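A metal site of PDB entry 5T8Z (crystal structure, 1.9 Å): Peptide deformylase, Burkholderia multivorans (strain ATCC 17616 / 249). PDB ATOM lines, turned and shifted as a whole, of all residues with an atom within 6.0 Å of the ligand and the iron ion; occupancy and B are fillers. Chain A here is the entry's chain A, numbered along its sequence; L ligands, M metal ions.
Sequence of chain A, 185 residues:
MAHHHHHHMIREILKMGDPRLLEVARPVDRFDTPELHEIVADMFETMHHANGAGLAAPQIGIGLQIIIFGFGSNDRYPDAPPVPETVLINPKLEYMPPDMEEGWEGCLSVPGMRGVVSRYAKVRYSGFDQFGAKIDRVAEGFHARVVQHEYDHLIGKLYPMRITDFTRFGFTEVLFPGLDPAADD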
ATOM      1  N   ALA A  50       3.762   6.851 -22.405  1.00  0.00           N
ATOM      2  CA  ALA A  50       3.202   5.583 -21.961  1.00  0.00           C
ATOM      3  C   ALA A  50       4.159   4.784 -21.074  1.00  0.00           C
ATOM      4  O   ALA A  50       3.825   3.647 -20.701  1.00  0.00           O
ATOM      5  CB  ALA A  50       2.772   4.750 -23.168  1.00  0.00           C
ATOM      6  N   ASN A  51       5.316   5.343 -20.725  1.00  0.00           N
ATOM      7  CA  ASN A  51       6.388   4.640 -20.023  1.00  0.00           C
ATOM      8  C   ASN A  51       6.763   3.339 -20.735  1.00  0.00           C
ATOM      9  O   ASN A  51       7.001   2.295 -20.123  1.00  0.00           O
ATOM     10  CB  ASN A  51       6.027   4.381 -18.556  1.00  0.00           C
ATOM     11  N   GLY A  52       6.829   3.404 -22.067  1.00  0.00           N
ATOM     12  CA  GLY A  52       7.232   2.254 -22.864  1.00  0.00           C
ATOM     13  C   GLY A  52       8.733   2.175 -23.021  1.00  0.00           C
ATOM     14  O   GLY A  52       9.446   3.171 -22.975  1.00  0.00           O
ATOM     15  N   ALA A  53       9.224   0.949 -23.200  1.00  0.00           N
ATOM     16  CA  ALA A  53      10.641   0.715 -23.433  1.00  0.00           C
ATOM     17  C   ALA A  53      10.979   0.662 -24.917  1.00  0.00           C
ATOM     18  O   ALA A  53      12.168   0.716 -25.264  1.00  0.00           O
ATOM     19  CB  ALA A  53      11.115  -0.566 -22.750  1.00  0.00           C
ATOM     20  N   GLY A  54       9.976   0.566 -25.784  1.00  0.00           N
ATOM     21  CA  GLY A  54      10.146   0.609 -27.223  1.00  0.00           C
ATOM     22  C   GLY A  54       8.841   0.989 -27.883  1.00  0.00           C
ATOM     23  O   GLY A  54       7.789   1.043 -27.238  1.00  0.00           O
ATOM     24  N   LEU A  55       8.909   1.279 -29.184  1.00  0.00           N
ATOM     25  CA  LEU A  55       7.732   1.573 -29.994  1.00  0.00           C
ATOM     26  C   LEU A  55       8.065   1.303 -31.460  1.00  0.00           C
ATOM     27  O   LEU A  55       9.190   1.545 -31.897  1.00  0.00           O
ATOM     28  CB  LEU A  55       7.259   3.023 -29.814  1.00  0.00           C
ATOM     29  CG  LEU A  55       5.836   3.356 -30.294  1.00  0.00           C
ATOM     30  CD1 LEU A  55       4.802   2.670 -29.388  1.00  0.00           C
ATOM     31  CD2 LEU A  55       5.533   4.854 -30.372  1.00  0.00           C
ATOM     32  N   ALA A  56       7.072   0.833 -32.198  1.00  0.00           N
ATOM     33  CA  ALA A  56       7.227   0.604 -33.633  1.00  0.00           C
ATOM     34  C   ALA A  56       6.245   1.477 -34.405  1.00  0.00           C
ATOM     35  O   ALA A  56       5.104   1.679 -33.956  1.00  0.00           O
ATOM     36  CB  ALA A  56       7.023  -0.904 -33.973  1.00  0.00           C
ATOM     37  N   GLN A  59       2.448   0.898 -34.796  1.00  0.00           N
ATOM     38  CA  GLN A  59       1.593   1.111 -33.623  1.00  0.00           C
ATOM     39  C   GLN A  59       0.988   2.508 -33.588  1.00  0.00           C
ATOM     40  O   GLN A  59      -0.007   2.721 -32.879  1.00  0.00           O
ATOM     41  CB  GLN A  59       2.374   0.878 -32.323  1.00  0.00           C
ATOM     42  CG  GLN A  59       2.901  -0.548 -32.108  1.00  0.00           C
ATOM     43  CD  GLN A  59       3.639  -0.656 -30.805  1.00  0.00           C
ATOM     44  OE1 GLN A  59       4.843  -0.350 -30.743  1.00  0.00           O
ATOM     45  NE2 GLN A  59       2.940  -1.057 -29.735  1.00  0.00           N
ATOM     46  N   TRP A 104       8.173 -12.174 -18.959  1.00  0.00           N
ATOM     47  CA  TRP A 104       6.907 -11.450 -19.041  1.00  0.00           C
ATOM     48  C   TRP A 104       7.020 -10.288 -20.017  1.00  0.00           C
ATOM     49  O   TRP A 104       7.989  -9.524 -19.963  1.00  0.00           O
ATOM     50  CB  TRP A 104       6.526 -10.913 -17.668  1.00  0.00           C
ATOM     51  CG  TRP A 104       6.121 -12.000 -16.727  1.00  0.00           C
ATOM     52  CD1 TRP A 104       6.889 -12.585 -15.757  1.00  0.00           C
ATOM     53  CD2 TRP A 104       4.860 -12.656 -16.693  1.00  0.00           C
ATOM     54  NE1 TRP A 104       6.169 -13.551 -15.099  1.00  0.00           N
ATOM     55  CE2 TRP A 104       4.906 -13.615 -15.656  1.00  0.00           C
ATOM     56  CE3 TRP A 104       3.669 -12.517 -17.425  1.00  0.00           C
ATOM     57  CZ2 TRP A 104       3.827 -14.424 -15.340  1.00  0.00           C
ATOM     58  CZ3 TRP A 104       2.601 -13.329 -17.115  1.00  0.00           C
ATOM     59  CH2 TRP A 104       2.685 -14.273 -16.077  1.00  0.00           C
ATOM     60  N   GLU A 105       6.042 -10.142 -20.914  1.00  0.00           N
ATOM     61  CA  GLU A 105       5.963  -8.990 -21.793  1.00  0.00           C
ATOM     62  C   GLU A 105       4.580  -8.359 -21.699  1.00  0.00           C
ATOM     63  O   GLU A 105       3.567  -9.037 -21.491  1.00  0.00           O
ATOM     64  CB  GLU A 105       6.255  -9.353 -23.251  1.00  0.00           C
ATOM     65  CG  GLU A 105       7.588 -10.073 -23.422  1.00  0.00           C
ATOM     66  CD  GLU A 105       8.038 -10.214 -24.880  1.00  0.00           C
ATOM     67  OE1 GLU A 105       7.429  -9.624 -25.800  1.00  0.00           O
ATOM     68  OE2 GLU A 105       9.031 -10.946 -25.097  1.00  0.00           O
ATOM     69  N   GLY A 106       4.542  -7.034 -21.832  1.00  0.00           N
ATOM     70  CA  GLY A 106       3.345  -6.307 -22.168  1.00  0.00           C
ATOM     71  C   GLY A 106       3.578  -5.516 -23.445  1.00  0.00           C
ATOM     72  O   GLY A 106       4.714  -5.350 -23.913  1.00  0.00           O
ATOM     73  N   CYS A 107       2.486  -5.010 -23.991  1.00  0.00           N
ATOM     74  CA  CYS A 107       2.488  -4.277 -25.250  1.00  0.00           C
ATOM     75  C   CYS A 107       1.561  -3.078 -25.116  1.00  0.00           C
ATOM     76  O   CYS A 107       0.451  -3.210 -24.602  1.00  0.00           O
ATOM     77  CB  CYS A 107       2.028  -5.166 -26.419  1.00  0.00           C
ATOM     78  SG  CYS A 107       2.173  -4.390 -28.063  1.00  0.00           S
ATOM     79  N   LEU A 108       2.022  -1.920 -25.591  1.00  0.00           N
ATOM     80  CA  LEU A 108       1.165  -0.751 -25.576  1.00  0.00           C
ATOM     81  C   LEU A 108      -0.066  -0.929 -26.468  1.00  0.00           C
ATOM     82  O   LEU A 108      -1.051  -0.209 -26.293  1.00  0.00           O
ATOM     83  CB  LEU A 108       1.962   0.474 -25.997  1.00  0.00           C
ATOM     84  CG  LEU A 108       3.006   0.869 -24.954  1.00  0.00           C
ATOM     85  CD1 LEU A 108       3.870   2.031 -25.434  1.00  0.00           C
ATOM     86  CD2 LEU A 108       2.306   1.208 -23.619  1.00  0.00           C
ATOM     87  N   SER A 109      -0.039  -1.892 -27.398  1.00  0.00           N
ATOM     88  CA  SER A 109      -1.189  -2.214 -28.225  1.00  0.00           C
ATOM     89  C   SER A 109      -2.086  -3.302 -27.615  1.00  0.00           C
ATOM     90  O   SER A 109      -3.128  -3.629 -28.182  1.00  0.00           O
ATOM     91  CB  SER A 109      -0.714  -2.676 -29.622  1.00  0.00           C
ATOM     92  OG  SER A 109      -0.046  -1.601 -30.301  1.00  0.00           O
ATOM     93  N   MET A 113      -2.547  -6.088 -20.063  1.00  0.00           N
ATOM     94  CA  MET A 113      -2.234  -7.509 -20.008  1.00  0.00           C
ATOM     95  C   MET A 113      -0.727  -7.756 -19.976  1.00  0.00           C
ATOM     96  O   MET A 113       0.084  -6.889 -20.321  1.00  0.00           O
ATOM     97  CB  MET A 113      -2.859  -8.228 -21.199  1.00  0.00           C
ATOM     98  CG  MET A 113      -4.326  -7.839 -21.380  1.00  0.00           C
ATOM     99  SD  MET A 113      -5.194  -8.962 -22.450  1.00  0.00           S
ATOM    100  CE  MET A 113      -5.400 -10.367 -21.336  1.00  0.00           C
ATOM    101  N   ARG A 114      -0.368  -8.970 -19.541  1.00  0.00           N
ATOM    102  CA  ARG A 114       0.991  -9.502 -19.613  1.00  0.00           C
ATOM    103  C   ARG A 114       0.930 -10.979 -20.013  1.00  0.00           C
ATOM    104  O   ARG A 114      -0.034 -11.680 -19.697  1.00  0.00           O
ATOM    105  CB  ARG A 114       1.736  -9.413 -18.268  1.00  0.00           C
ATOM    106  CG  ARG A 114       1.844  -8.010 -17.686  1.00  0.00           C
ATOM    107  CD  ARG A 114       2.862  -7.200 -18.520  1.00  0.00           C
ATOM    108  NE  ARG A 114       3.188  -5.918 -17.876  1.00  0.00           N
ATOM    109  CZ  ARG A 114       2.604  -4.763 -18.171  1.00  0.00           C
ATOM    110  NH1 ARG A 114       1.638  -4.717 -19.096  1.00  0.00           N
ATOM    111  NH2 ARG A 114       2.977  -3.643 -17.545  1.00  0.00           N
ATOM    112  N   PHE A 142      17.367  -8.537 -21.867  1.00  0.00           N
ATOM    113  CA  PHE A 142      16.240  -7.619 -22.053  1.00  0.00           C
ATOM    114  C   PHE A 142      16.425  -6.746 -23.294  1.00  0.00           C
ATOM    115  O   PHE A 142      15.482  -6.523 -24.054  1.00  0.00           O
ATOM    116  CB  PHE A 142      16.066  -6.742 -20.797  1.00  0.00           C
ATOM    117  CG  PHE A 142      14.870  -5.823 -20.875  1.00  0.00           C
ATOM    118  CD1 PHE A 142      13.583  -6.325 -20.743  1.00  0.00           C
ATOM    119  CD2 PHE A 142      15.038  -4.469 -21.106  1.00  0.00           C
ATOM    120  CE1 PHE A 142      12.479  -5.489 -20.820  1.00  0.00           C
ATOM    121  CE2 PHE A 142      13.939  -3.620 -21.180  1.00  0.00           C
ATOM    122  CZ  PHE A 142      12.663  -4.136 -21.034  1.00  0.00           C
ATOM    123  N   ARG A 145      15.404  -8.806 -26.027  1.00  0.00           N
ATOM    124  CA  ARG A 145      13.959  -9.023 -25.971  1.00  0.00           C
ATOM    125  C   ARG A 145      13.199  -7.839 -26.558  1.00  0.00           C
ATOM    126  O   ARG A 145      12.291  -8.010 -27.388  1.00  0.00           O
ATOM    127  CB  ARG A 145      13.530  -9.273 -24.530  1.00  0.00           C
ATOM    128  CG  ARG A 145      11.996  -9.429 -24.360  1.00  0.00           C
ATOM    129  CD  ARG A 145      11.639  -9.870 -22.957  1.00  0.00           C
ATOM    130  NE  ARG A 145      12.226 -11.175 -22.647  1.00  0.00           N
ATOM    131  CZ  ARG A 145      11.624 -12.347 -22.821  1.00  0.00           C
ATOM    132  NH1 ARG A 145      10.375 -12.424 -23.297  1.00  0.00           N
ATOM    133  NH2 ARG A 145      12.289 -13.463 -22.490  1.00  0.00           N
ATOM    134  N   VAL A 146      13.550  -6.612 -26.136  1.00  0.00           N
ATOM    135  CA  VAL A 146      12.861  -5.451 -26.669  1.00  0.00           C
ATOM    136  C   VAL A 146      12.997  -5.396 -28.180  1.00  0.00           C
ATOM    137  O   VAL A 146      12.018  -5.151 -28.896  1.00  0.00           O
ATOM    138  CB  VAL A 146      13.394  -4.148 -26.035  1.00  0.00           C
ATOM    139  CG1 VAL A 146      12.757  -2.950 -26.713  1.00  0.00           C
ATOM    140  CG2 VAL A 146      13.086  -4.113 -24.558  1.00  0.00           C
ATOM    141  N   HIS A 149      10.715  -7.911 -29.801  1.00  0.00           N
ATOM    142  CA  HIS A 149       9.321  -7.484 -29.671  1.00  0.00           C
ATOM    143  C   HIS A 149       8.978  -6.390 -30.676  1.00  0.00           C
ATOM    144  O   HIS A 149       7.932  -6.446 -31.330  1.00  0.00           O
ATOM    145  CB  HIS A 149       9.125  -7.013 -28.250  1.00  0.00           C
ATOM    146  CG  HIS A 149       7.749  -6.523 -27.946  1.00  0.00           C
ATOM    147  ND1 HIS A 149       6.885  -7.220 -27.136  1.00  0.00           N
ATOM    148  CD2 HIS A 149       7.094  -5.413 -28.352  1.00  0.00           C
ATOM    149  CE1 HIS A 149       5.755  -6.538 -27.028  1.00  0.00           C
ATOM    150  NE2 HIS A 149       5.856  -5.445 -27.762  1.00  0.00           N
ATOM    151  N   GLU A 150       9.846  -5.374 -30.822  1.00  0.00           N
ATOM    152  CA  GLU A 150       9.540  -4.299 -31.758  1.00  0.00           C
ATOM    153  C   GLU A 150       9.663  -4.769 -33.194  1.00  0.00           C
ATOM    154  O   GLU A 150       8.848  -4.372 -34.050  1.00  0.00           O
ATOM    155  CB  GLU A 150      10.460  -3.092 -31.532  1.00  0.00           C
ATOM    156  CG  GLU A 150      10.425  -2.555 -30.109  1.00  0.00           C
ATOM    157  CD  GLU A 150       9.035  -2.142 -29.645  1.00  0.00           C
ATOM    158  OE1 GLU A 150       8.150  -1.837 -30.469  1.00  0.00           O
ATOM    159  OE2 GLU A 150       8.839  -2.115 -28.410  1.00  0.00           O
ATOM    160  N   HIS A 153       6.569  -6.311 -34.499  1.00  0.00           N
ATOM    161  CA  HIS A 153       5.541  -5.368 -34.956  1.00  0.00           C
ATOM    162  C   HIS A 153       5.681  -5.051 -36.436  1.00  0.00           C
ATOM    163  O   HIS A 153       4.686  -4.749 -37.091  1.00  0.00           O
ATOM    164  CB  HIS A 153       5.574  -4.059 -34.159  1.00  0.00           C
ATOM    165  CG  HIS A 153       4.835  -4.143 -32.874  1.00  0.00           C
ATOM    166  ND1 HIS A 153       3.486  -4.430 -32.813  1.00  0.00           N
ATOM    167  CD2 HIS A 153       5.239  -3.985 -31.592  1.00  0.00           C
ATOM    168  CE1 HIS A 153       3.099  -4.425 -31.552  1.00  0.00           C
ATOM    169  NE2 HIS A 153       4.143  -4.172 -30.795  1.00  0.00           N
ATOM    170  N   TYR A 159       2.643 -10.041 -29.438  1.00  0.00           N
ATOM    171  CA  TYR A 159       3.226 -11.098 -28.610  1.00  0.00           C
ATOM    172  C   TYR A 159       2.258 -12.233 -28.270  1.00  0.00           C
ATOM    173  O   TYR A 159       2.745 -13.366 -28.098  1.00  0.00           O
ATOM    174  CB  TYR A 159       3.889 -10.501 -27.341  1.00  0.00           C
ATOM    175  CG  TYR A 159       2.908 -10.102 -26.233  1.00  0.00           C
ATOM    176  CD1 TYR A 159       2.479 -11.040 -25.299  1.00  0.00           C
ATOM    177  CD2 TYR A 159       2.416  -8.806 -26.144  1.00  0.00           C
ATOM    178  CE1 TYR A 159       1.541 -10.696 -24.285  1.00  0.00           C
ATOM    179  CE2 TYR A 159       1.513  -8.433 -25.111  1.00  0.00           C
ATOM    180  CZ  TYR A 159       1.070  -9.394 -24.191  1.00  0.00           C
ATOM    181  OH  TYR A 159       0.166  -9.036 -23.197  1.00  0.00           O
ATOM    182  N   PHE A 176       0.135  -9.186 -11.247  1.00  0.00           N
ATOM    183  CA  PHE A 176       1.099  -8.406 -10.459  1.00  0.00           C
ATOM    184  C   PHE A 176       0.390  -7.270  -9.722  1.00  0.00           C
ATOM    185  O   PHE A 176       0.444  -6.112 -10.154  1.00  0.00           O
ATOM    186  CB  PHE A 176       2.204  -7.849 -11.360  1.00  0.00           C
ATOM    187  CG  PHE A 176       2.808  -8.841 -12.321  1.00  0.00           C
ATOM    188  CD1 PHE A 176       3.933  -9.596 -11.965  1.00  0.00           C
ATOM    189  CD2 PHE A 176       2.316  -8.971 -13.615  1.00  0.00           C
ATOM    190  CE1 PHE A 176       4.524 -10.477 -12.873  1.00  0.00           C
ATOM    191  CE2 PHE A 176       2.896  -9.853 -14.529  1.00  0.00           C
ATOM    192  CZ  PHE A 176       4.000 -10.604 -14.152  1.00  0.00           C
HETATM  193  C1  LIG L   1       6.191  -1.457 -25.415  1.00  0.00           C
HETATM  194  C2  LIG L   1       5.598  -1.830 -26.761  1.00  0.00           C
HETATM  195  O1  LIG L   1       4.419  -2.144 -26.882  1.00  0.00           O
HETATM  196  N1  LIG L   1       6.447  -1.769 -27.771  1.00  0.00           N
HETATM  197  O2  LIG L   1       6.069  -2.244 -29.025  1.00  0.00           O
HETATM  198  C3  LIG L   1       6.812  -2.643 -24.681  1.00  0.00           C
HETATM  199  C4  LIG L   1       6.987  -2.286 -23.225  1.00  0.00           C
HETATM  200  O3  LIG L   1       7.677  -1.328 -22.864  1.00  0.00           O
HETATM  201  C5  LIG L   1       8.197  -2.913 -25.287  1.00  0.00           C
HETATM  202  C6  LIG L   1       9.034  -3.961 -24.549  1.00  0.00           C
HETATM  203  C7  LIG L   1       8.521  -5.379 -24.709  1.00  0.00           C
HETATM  204  C8  LIG L   1       9.388  -6.422 -24.028  1.00  0.00           C
HETATM  205  C9  LIG L   1       9.368  -6.328 -22.524  1.00  0.00           C
HETATM  206  N2  LIG L   1       6.357  -3.094 -22.357  1.00  0.00           N
HETATM  207  C10 LIG L   1       6.532  -2.941 -20.925  1.00  0.00           C
HETATM  208  C11 LIG L   1       5.299  -2.303 -20.256  1.00  0.00           C
HETATM  209  C12 LIG L   1       5.297  -0.801 -20.422  1.00  0.00           C
HETATM  210  C13 LIG L   1       4.000  -2.896 -20.796  1.00  0.00           C
HETATM  211  C14 LIG L   1       6.912  -4.294 -20.318  1.00  0.00           C
HETATM  212  O4  LIG L   1       6.505  -5.329 -20.833  1.00  0.00           O
HETATM  213  N3  LIG L   1       7.725  -4.298 -19.249  1.00  0.00           N
HETATM  214  C15 LIG L   1       8.133  -5.560 -18.611  1.00  0.00           C
HETATM  215  C16 LIG L   1       8.324  -3.133 -18.598  1.00  0.00           C
HETATM  216  C17 LIG L   1       9.582  -3.691 -18.003  1.00  0.00           C
HETATM  217  C18 LIG L   1       9.211  -5.117 -17.611  1.00  0.00           C
HETATM  218  C19 LIG L   1       6.947  -6.259 -17.942  1.00  0.00           C
HETATM  219  O5  LIG L   1       7.373  -7.367 -17.169  1.00  0.00           O
HETATM  220 FE    FE M   1       4.438  -3.862 -28.520  1.00  0.00          FE
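The side-chain carboxylate of Glu 150 is in hydrogen-bond range of a nitrogen (N1) of the ligand (2.5 Å).
O of Gly 54 lies within hydrogen-bond range of N1 of the ligand, at 3.2 Å.
The side-chain amide oxygen (OE1) of Gln 59 lies close to an oxygen (O2) of the ligand, 2.8 Å away.
O1 of the ligand lies close to N of Leu 108, 2.7 Å away.
O3 of the ligand lies within hydrogen-bond range of N of Ala 53 (2.8 Å).
O4 of the ligand lies within hydrogen-bond range of N of Gly 106.
N2 of the ligand sits at hydrogen-bond distance from O of Gly 106 (3.2 Å).
OE2 of Glu 105 is in salt-bridge range of NH1 of Arg 145 (2.7 Å).
The backbone NH (N) of Ser 109 sits close to the side-chain sulfur (SG) of Cys 107 (3.4 Å).
The side-chain amide oxygen of Gln 59 sits at hydrogen-bond distance from the backbone NH of Ala 56, 2.9 Å away.
NE2 of Gln 59 sits at hydrogen-bond distance from OG of Ser 109 (3.1 Å).
OE1 of Glu 150 sits close to N of Leu 55, 3.5 Å away.
The side-chain carboxylate of Glu 150 lies within hydrogen-bond range of the backbone NH of Ala 56 (3.4 Å).
The side-chain carboxylate (OE1) of Glu 105 is in hydrogen-bond range of a ring nitrogen (ND1) of His 149, at 2.8 Å.
Asn 51 touches the ligand.
CA of Gly 52 touches O3 of the ligand, at 3.6 Å.
Trp 104 touches the ligand.
Glu 105 touches the ligand (C to O4, 3.7 Å).
Arg 114 touches the ligand.
Phe 142 touches the ligand.
Arg 145 touches the ligand (CG to C8, 3.99 Å).
Hydrophobic or aromatic side chains that line the ligand: Ala 53, Trp 104, Leu 108, Phe 142, His 149 and His 153.
Of the 24 residues printed, 16 come within 4 Å of the ligand.
The nearest printed residue that does not touch the ligand is Val 146 (4.1 Å).
The iron ion is bound by a ring nitrogen (NE2) of His 149, a ring nitrogen (NE2) of His 153, an oxygen (O2) of the ligand, the side-chain sulfur of Cys 107 and an oxygen (O1) of the ligand.
The iron ion has five donor atoms within binding distance.
Merely in contact with the iron ion: Gln 59.
Of the 24 residues printed, 4 come within 4 Å of the iron ion.
The nearest printed residue that does not touch the iron ion is Leu 108 (4.3 Å).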
